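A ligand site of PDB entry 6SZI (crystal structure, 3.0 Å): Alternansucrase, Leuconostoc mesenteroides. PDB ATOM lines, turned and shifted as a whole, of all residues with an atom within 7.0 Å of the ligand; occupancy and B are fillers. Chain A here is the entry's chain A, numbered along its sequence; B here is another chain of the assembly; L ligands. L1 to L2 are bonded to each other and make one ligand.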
ATOM      1  N   TYR A  95      21.923   8.117  16.558  1.00  0.00           N
ATOM      2  CA  TYR A  95      22.959   8.938  15.944  1.00  0.00           C
ATOM      3  C   TYR A  95      22.742  10.372  16.393  1.00  0.00           C
ATOM      4  O   TYR A  95      21.595  10.777  16.537  1.00  0.00           O
ATOM      5  CB  TYR A  95      22.850   8.894  14.409  1.00  0.00           C
ATOM      6  CG  TYR A  95      23.313   7.591  13.768  1.00  0.00           C
ATOM      7  CD1 TYR A  95      24.677   7.270  13.692  1.00  0.00           C
ATOM      8  CD2 TYR A  95      22.403   6.703  13.208  1.00  0.00           C
ATOM      9  CE1 TYR A  95      25.102   6.094  13.097  1.00  0.00           C
ATOM     10  CE2 TYR A  95      22.821   5.530  12.601  1.00  0.00           C
ATOM     11  CZ  TYR A  95      24.174   5.231  12.554  1.00  0.00           C
ATOM     12  OH  TYR A  95      24.591   4.067  11.967  1.00  0.00           O
ATOM     13  N   VAL A  96      23.822  11.117  16.630  1.00  0.00           N
ATOM     14  CA  VAL A  96      23.720  12.596  16.678  1.00  0.00           C
ATOM     15  C   VAL A  96      24.889  13.271  15.977  1.00  0.00           C
ATOM     16  O   VAL A  96      26.046  12.830  16.084  1.00  0.00           O
ATOM     17  CB  VAL A  96      23.670  13.178  18.087  1.00  0.00           C
ATOM     18  CG1 VAL A  96      23.098  14.593  18.021  1.00  0.00           C
ATOM     19  CG2 VAL A  96      22.859  12.290  19.031  1.00  0.00           C
ATOM     20  N   ALA A  97      24.561  14.327  15.243  1.00  0.00           N
ATOM     21  CA  ALA A  97      25.553  15.132  14.583  1.00  0.00           C
ATOM     22  C   ALA A  97      25.774  16.340  15.467  1.00  0.00           C
ATOM     23  O   ALA A  97      24.807  16.921  15.940  1.00  0.00           O
ATOM     24  CB  ALA A  97      25.064  15.561  13.200  1.00  0.00           C
ATOM     25  N   GLY A 101      29.171  19.177  12.395  1.00  0.00           N
ATOM     26  CA  GLY A 101      28.645  18.220  11.422  1.00  0.00           C
ATOM     27  C   GLY A 101      29.271  16.837  11.533  1.00  0.00           C
ATOM     28  O   GLY A 101      29.102  16.047  10.613  1.00  0.00           O
ATOM     29  N   GLN A 102      29.977  16.562  12.629  1.00  0.00           N
ATOM     30  CA  GLN A 102      30.497  15.228  12.943  1.00  0.00           C
ATOM     31  C   GLN A 102      29.455  14.340  13.617  1.00  0.00           C
ATOM     32  O   GLN A 102      28.633  14.816  14.405  1.00  0.00           O
ATOM     33  CB  GLN A 102      31.691  15.320  13.891  1.00  0.00           C
ATOM     34  CG  GLN A 102      32.908  15.988  13.302  1.00  0.00           C
ATOM     35  CD  GLN A 102      33.967  16.221  14.354  1.00  0.00           C
ATOM     36  OE1 GLN A 102      35.090  15.763  14.217  1.00  0.00           O
ATOM     37  NE2 GLN A 102      33.591  16.921  15.426  1.00  0.00           N
ATOM     38  N   THR A 103      29.546  13.030  13.371  1.00  0.00           N
ATOM     39  CA  THR A 103      28.491  12.117  13.772  1.00  0.00           C
ATOM     40  C   THR A 103      29.001  11.041  14.724  1.00  0.00           C
ATOM     41  O   THR A 103      30.024  10.393  14.476  1.00  0.00           O
ATOM     42  CB  THR A 103      27.876  11.465  12.530  1.00  0.00           C
ATOM     43  OG1 THR A 103      27.400  12.485  11.653  1.00  0.00           O
ATOM     44  CG2 THR A 103      26.721  10.592  12.923  1.00  0.00           C
ATOM     45  N   TYR A 104      28.270  10.871  15.830  1.00  0.00           N
ATOM     46  CA  TYR A 104      28.553   9.839  16.836  1.00  0.00           C
ATOM     47  C   TYR A 104      27.351   8.918  16.885  1.00  0.00           C
ATOM     48  O   TYR A 104      26.224   9.335  16.590  1.00  0.00           O
ATOM     49  CB  TYR A 104      28.708  10.447  18.229  1.00  0.00           C
ATOM     50  CG  TYR A 104      29.790  11.475  18.390  1.00  0.00           C
ATOM     51  CD1 TYR A 104      29.617  12.775  17.950  1.00  0.00           C
ATOM     52  CD2 TYR A 104      30.989  11.150  19.002  1.00  0.00           C
ATOM     53  CE1 TYR A 104      30.615  13.718  18.102  1.00  0.00           C
ATOM     54  CE2 TYR A 104      31.985  12.089  19.171  1.00  0.00           C
ATOM     55  CZ  TYR A 104      31.793  13.372  18.711  1.00  0.00           C
ATOM     56  OH  TYR A 104      32.800  14.302  18.856  1.00  0.00           O
ATOM     57  N   ASP A 120      21.737  -1.167  12.066  1.00  0.00           N
ATOM     58  CA  ASP A 120      20.658  -1.437  11.075  1.00  0.00           C
ATOM     59  C   ASP A 120      21.205  -2.274   9.905  1.00  0.00           C
ATOM     60  O   ASP A 120      20.832  -2.046   8.761  1.00  0.00           O
ATOM     61  CB  ASP A 120      20.026  -0.154  10.510  1.00  0.00           C
ATOM     62  CG  ASP A 120      19.632   0.846  11.580  1.00  0.00           C
ATOM     63  OD1 ASP A 120      19.136   0.425  12.639  1.00  0.00           O
ATOM     64  OD2 ASP A 120      19.826   2.062  11.345  1.00  0.00           O
ATOM     65  N   ASN A 122      24.223  -2.109   8.702  1.00  0.00           N
ATOM     66  CA  ASN A 122      25.214  -1.315   7.973  1.00  0.00           C
ATOM     67  C   ASN A 122      26.538  -1.397   8.712  1.00  0.00           C
ATOM     68  O   ASN A 122      26.580  -1.259   9.944  1.00  0.00           O
ATOM     69  CB  ASN A 122      24.804   0.150   7.881  1.00  0.00           C
ATOM     70  CG  ASN A 122      23.529   0.372   7.077  1.00  0.00           C
ATOM     71  OD1 ASN A 122      23.444   1.299   6.274  1.00  0.00           O
ATOM     72  ND2 ASN A 122      22.529  -0.442   7.325  1.00  0.00           N
ATOM     73  N   GLN A 124      29.966   0.260   9.707  1.00  0.00           N
ATOM     74  CA  GLN A 124      30.513   1.621   9.862  1.00  0.00           C
ATOM     75  C   GLN A 124      31.774   1.634  10.744  1.00  0.00           C
ATOM     76  O   GLN A 124      32.025   0.671  11.488  1.00  0.00           O
ATOM     77  CB  GLN A 124      29.443   2.548  10.441  1.00  0.00           C
ATOM     78  CG  GLN A 124      28.263   2.753   9.506  1.00  0.00           C
ATOM     79  CD  GLN A 124      27.034   3.298  10.206  1.00  0.00           C
ATOM     80  OE1 GLN A 124      26.923   3.264  11.427  1.00  0.00           O
ATOM     81  NE2 GLN A 124      26.098   3.824   9.410  1.00  0.00           N
ATOM     82  N   PHE A 126      34.392   4.009  13.446  1.00  0.00           N
ATOM     83  CA  PHE A 126      34.484   5.153  14.352  1.00  0.00           C
ATOM     84  C   PHE A 126      35.914   5.326  14.901  1.00  0.00           C
ATOM     85  O   PHE A 126      36.525   4.358  15.352  1.00  0.00           O
ATOM     86  CB  PHE A 126      33.484   4.986  15.508  1.00  0.00           C
ATOM     87  CG  PHE A 126      32.052   5.107  15.096  1.00  0.00           C
ATOM     88  CD1 PHE A 126      31.330   3.989  14.687  1.00  0.00           C
ATOM     89  CD2 PHE A 126      31.412   6.320  15.132  1.00  0.00           C
ATOM     90  CE1 PHE A 126      29.993   4.101  14.303  1.00  0.00           C
ATOM     91  CE2 PHE A 126      30.087   6.439  14.751  1.00  0.00           C
ATOM     92  CZ  PHE A 126      29.370   5.331  14.333  1.00  0.00           C
ATOM     93  N   GLN A 132      32.404   9.426  13.527  1.00  0.00           N
ATOM     94  CA  GLN A 132      32.120   8.549  12.383  1.00  0.00           C
ATOM     95  C   GLN A 132      32.888   8.965  11.148  1.00  0.00           C
ATOM     96  O   GLN A 132      32.769  10.109  10.686  1.00  0.00           O
ATOM     97  CB  GLN A 132      30.621   8.526  12.046  1.00  0.00           C
ATOM     98  CG  GLN A 132      30.258   7.343  11.155  1.00  0.00           C
ATOM     99  CD  GLN A 132      28.811   7.315  10.696  1.00  0.00           C
ATOM    100  OE1 GLN A 132      28.023   8.215  10.979  1.00  0.00           O
ATOM    101  NE2 GLN A 132      28.464   6.260   9.955  1.00  0.00           N
ATOM    102  N   LYS A 134      33.366   9.166   7.353  1.00  0.00           N
ATOM    103  CA  LYS A 134      32.539   9.311   6.166  1.00  0.00           C
ATOM    104  C   LYS A 134      33.410   9.812   5.020  1.00  0.00           C
ATOM    105  O   LYS A 134      34.219  10.728   5.195  1.00  0.00           O
ATOM    106  CB  LYS A 134      31.414  10.298   6.435  1.00  0.00           C
ATOM    107  CG  LYS A 134      30.326   9.749   7.348  1.00  0.00           C
ATOM    108  CD  LYS A 134      29.159  10.711   7.484  1.00  0.00           C
ATOM    109  CE  LYS A 134      28.071  10.162   8.397  1.00  0.00           C
ATOM    110  NZ  LYS A 134      26.900  11.081   8.450  1.00  0.00           N
ATOM    111  N   PRO A 149      30.195   8.823   1.695  1.00  0.00           N
ATOM    112  CA  PRO A 149      30.128  10.238   2.014  1.00  0.00           C
ATOM    113  C   PRO A 149      29.120  10.654   3.062  1.00  0.00           C
ATOM    114  O   PRO A 149      29.451  11.471   3.932  1.00  0.00           O
ATOM    115  CB  PRO A 149      29.735  10.868   0.672  1.00  0.00           C
ATOM    116  CG  PRO A 149      30.372   9.995  -0.333  1.00  0.00           C
ATOM    117  CD  PRO A 149      30.490   8.624   0.268  1.00  0.00           C
ATOM    118  N   ASN A 150      27.891  10.163   2.974  1.00  0.00           N
ATOM    119  CA  ASN A 150      26.863  10.676   3.877  1.00  0.00           C
ATOM    120  C   ASN A 150      26.302   9.682   4.862  1.00  0.00           C
ATOM    121  O   ASN A 150      26.055  10.016   6.024  1.00  0.00           O
ATOM    122  CB  ASN A 150      25.757  11.344   3.073  1.00  0.00           C
ATOM    123  CG  ASN A 150      26.232  12.634   2.437  1.00  0.00           C
ATOM    124  OD1 ASN A 150      26.950  13.405   3.055  1.00  0.00           O
ATOM    125  ND2 ASN A 150      25.856  12.848   1.175  1.00  0.00           N
ATOM    126  N   THR A 151      26.122   8.466   4.401  1.00  0.00           N
ATOM    127  CA  THR A 151      25.664   7.416   5.265  1.00  0.00           C
ATOM    128  C   THR A 151      26.816   6.933   6.117  1.00  0.00           C
ATOM    129  O   THR A 151      26.642   6.617   7.275  1.00  0.00           O
ATOM    130  CB  THR A 151      25.140   6.234   4.455  1.00  0.00           C
ATOM    131  OG1 THR A 151      26.210   5.645   3.700  1.00  0.00           O
ATOM    132  CG2 THR A 151      24.000   6.671   3.526  1.00  0.00           C
ATOM    133  N   GLY A 152      28.003   6.877   5.504  1.00  0.00           N
ATOM    134  CA  GLY A 152      29.194   6.330   6.153  1.00  0.00           C
ATOM    135  C   GLY A 152      29.154   4.822   6.109  1.00  0.00           C
ATOM    136  O   GLY A 152      29.909   4.177   6.832  1.00  0.00           O
ATOM    137  N   ASN A 153      28.322   4.257   5.234  1.00  0.00           N
ATOM    138  CA  ASN A 153      28.211   2.798   5.086  1.00  0.00           C
ATOM    139  C   ASN A 153      29.328   2.213   4.205  1.00  0.00           C
ATOM    140  O   ASN A 153      29.823   2.873   3.293  1.00  0.00           O
ATOM    141  CB  ASN A 153      26.842   2.439   4.521  1.00  0.00           C
ATOM    142  CG  ASN A 153      25.695   2.978   5.355  1.00  0.00           C
ATOM    143  OD1 ASN A 153      25.844   3.226   6.557  1.00  0.00           O
ATOM    144  ND2 ASN A 153      24.549   3.157   4.743  1.00  0.00           N
ATOM    145  N   ALA B 148      19.016  17.613   0.044  1.00  0.00           N
ATOM    146  CA  ALA B 148      20.316  17.093   0.449  1.00  0.00           C
ATOM    147  C   ALA B 148      20.701  15.816  -0.291  1.00  0.00           C
ATOM    148  O   ALA B 148      19.858  15.061  -0.688  1.00  0.00           O
ATOM    149  CB  ALA B 148      20.326  16.850   1.938  1.00  0.00           C
ATOM    150  N   PRO B 149      22.013  15.606  -0.484  1.00  0.00           N
ATOM    151  CA  PRO B 149      22.559  14.444  -1.191  1.00  0.00           C
ATOM    152  C   PRO B 149      21.984  13.054  -0.817  1.00  0.00           C
ATOM    153  O   PRO B 149      21.693  12.238  -1.717  1.00  0.00           O
ATOM    154  CB  PRO B 149      24.036  14.483  -0.804  1.00  0.00           C
ATOM    155  CG  PRO B 149      24.345  15.927  -0.628  1.00  0.00           C
ATOM    156  CD  PRO B 149      23.058  16.609  -0.225  1.00  0.00           C
ATOM    157  N   ASN B 150      21.869  12.778   0.467  1.00  0.00           N
ATOM    158  CA  ASN B 150      21.494  11.442   0.912  1.00  0.00           C
ATOM    159  C   ASN B 150      20.075  11.406   1.405  1.00  0.00           C
ATOM    160  O   ASN B 150      19.292  10.586   0.976  1.00  0.00           O
ATOM    161  CB  ASN B 150      22.449  10.978   2.003  1.00  0.00           C
ATOM    162  CG  ASN B 150      21.894   9.849   2.833  1.00  0.00           C
ATOM    163  OD1 ASN B 150      21.054   9.088   2.376  1.00  0.00           O
ATOM    164  ND2 ASN B 150      22.390   9.711   4.082  1.00  0.00           N
ATOM    165  N   THR B 151      19.747  12.303   2.312  1.00  0.00           N
ATOM    166  CA  THR B 151      18.398  12.338   2.869  1.00  0.00           C
ATOM    167  C   THR B 151      17.428  12.925   1.869  1.00  0.00           C
ATOM    168  O   THR B 151      16.272  12.499   1.807  1.00  0.00           O
ATOM    169  CB  THR B 151      18.347  13.200   4.128  1.00  0.00           C
ATOM    170  OG1 THR B 151      18.731  14.531   3.785  1.00  0.00           O
ATOM    171  CG2 THR B 151      19.309  12.665   5.213  1.00  0.00           C
ATOM    172  N   ASN B 153      16.585  15.823   2.228  1.00  0.00           N
ATOM    173  CA  ASN B 153      15.851  16.762   3.063  1.00  0.00           C
ATOM    174  C   ASN B 153      16.168  18.203   2.663  1.00  0.00           C
ATOM    175  O   ASN B 153      17.284  18.504   2.224  1.00  0.00           O
ATOM    176  CB  ASN B 153      16.184  16.521   4.541  1.00  0.00           C
ATOM    177  CG  ASN B 153      15.870  15.095   4.994  1.00  0.00           C
ATOM    178  OD1 ASN B 153      14.997  14.448   4.436  1.00  0.00           O
ATOM    179  ND2 ASN B 153      16.548  14.638   6.033  1.00  0.00           N
ATOM    180  N   VAL B 183      25.870  23.506   1.812  1.00  0.00           N
ATOM    181  CA  VAL B 183      25.914  22.079   2.125  1.00  0.00           C
ATOM    182  C   VAL B 183      27.248  21.665   2.712  1.00  0.00           C
ATOM    183  O   VAL B 183      27.280  20.851   3.616  1.00  0.00           O
ATOM    184  CB  VAL B 183      25.576  21.214   0.881  1.00  0.00           C
ATOM    185  CG1 VAL B 183      25.962  19.744   1.076  1.00  0.00           C
ATOM    186  CG2 VAL B 183      24.096  21.304   0.587  1.00  0.00           C
HETATM  187  C1  LIG L   1      25.989  13.955   8.036  1.00  0.00           C
HETATM  188  C2  LIG L   1      25.583  13.770   6.570  1.00  0.00           C
HETATM  189  C3  LIG L   1      24.057  13.749   6.421  1.00  0.00           C
HETATM  190  C4  LIG L   1      23.442  12.761   7.413  1.00  0.00           C
HETATM  191  C5  LIG L   1      23.995  12.985   8.842  1.00  0.00           C
HETATM  192  C6  LIG L   1      23.467  11.936   9.811  1.00  0.00           C
HETATM  193  O1  LIG L   1      25.531  15.205   8.519  1.00  0.00           O
HETATM  194  O2  LIG L   1      26.143  14.783   5.764  1.00  0.00           O
HETATM  195  O3  LIG L   1      23.707  13.319   5.134  1.00  0.00           O
HETATM  196  O4  LIG L   1      22.032  12.873   7.368  1.00  0.00           O
HETATM  197  O5  LIG L   1      25.410  12.926   8.823  1.00  0.00           O
HETATM  198  O6  LIG L   1      23.978  10.672   9.469  1.00  0.00           O
HETATM  199  C1  LG2 L   2      23.515   9.691  10.404  1.00  0.00           C
HETATM  200  C2  LG2 L   2      24.342   8.426  10.168  1.00  0.00           C
HETATM  201  C3  LG2 L   2      23.976   7.737   8.871  1.00  0.00           C
HETATM  202  C4  LG2 L   2      22.455   7.613   8.750  1.00  0.00           C
HETATM  203  C5  LG2 L   2      21.818   8.990   8.943  1.00  0.00           C
HETATM  204  C6  LG2 L   2      20.297   9.011   8.662  1.00  0.00           C
HETATM  205  O1  LG2 L   2      25.722   8.734  10.174  1.00  0.00           O
HETATM  206  O2  LG2 L   2      24.571   6.462   8.819  1.00  0.00           O
HETATM  207  O3  LG2 L   2      22.184   7.150   7.452  1.00  0.00           O
HETATM  208  O4  LG2 L   2      22.128   9.433  10.265  1.00  0.00           O
HETATM  209  O5  LG2 L   2      19.673   8.174   9.608  1.00  0.00           O
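NZ of Lys 134 lies within hydrogen-bond range of O5 of LIG L1 (2.4 Å).
The side-chain amide oxygen (OE1) of Gln 132 sits at hydrogen-bond distance from an oxygen (O1) of LG2 L2.
O of Thr 151 of chain A is in hydrogen-bond range of O2 of LG2 L2, 2.6 Å away.
An oxygen (O2) of LG2 L2 sits at hydrogen-bond distance from the side-chain amide nitrogen of Gln 124 (3.1 Å).
The side-chain amide oxygen (OD1) of Asn 150 of chain A is in hydrogen-bond range of an oxygen (O2) of LIG L1.
OG1 of Thr 103 is in hydrogen-bond range of O5 of LIG L1, 3.5 Å away.
NZ of Lys 134 sits at hydrogen-bond distance from O of Asn 150 of chain A, at 2.8 Å.
The side-chain amide nitrogen (NE2) of Gln 132 lies within hydrogen-bond range of the backbone carbonyl oxygen (O) of Thr 151 of chain A, 3.3 Å away.
NE2 of Gln 132 sits close to NE2 of Gln 124.
The backbone carbonyl oxygen (O) of Thr 103 sits at hydrogen-bond distance from the backbone NH (N) of Gln 132.
The side-chain hydroxyl of Thr 151 of chain A sits at hydrogen-bond distance from the backbone NH of Asn 153 of chain A (3.0 Å).
OE1 of Gln 124 lies within hydrogen-bond range of OH of Tyr 95 (2.5 Å).
The side-chain amide nitrogen (NE2) of Gln 124 is in hydrogen-bond range of the side-chain amide oxygen (OD1) of Asn 153 of chain A (2.9 Å).
CD1 of Tyr 95 touches C2 of LG2 L2, 3.7 Å away.
ND2 of Asn 150 of chain B touches O3 of LIG L1, 3.98 Å away.
CG2 of Thr 151 of chain B touches O4 of LIG L1, at 3.5 Å.
Hydrophobic or aromatic side chains that line the ligand: Tyr 95.
Nine residues have an atom within 4 Å of the ligand: Tyr 95, Thr 103, Gln 124, Gln 132, Lys 134, Asn 150 of chain A, Thr 151 of chain A, Asn 150 of chain B and Thr 151 of chain B.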
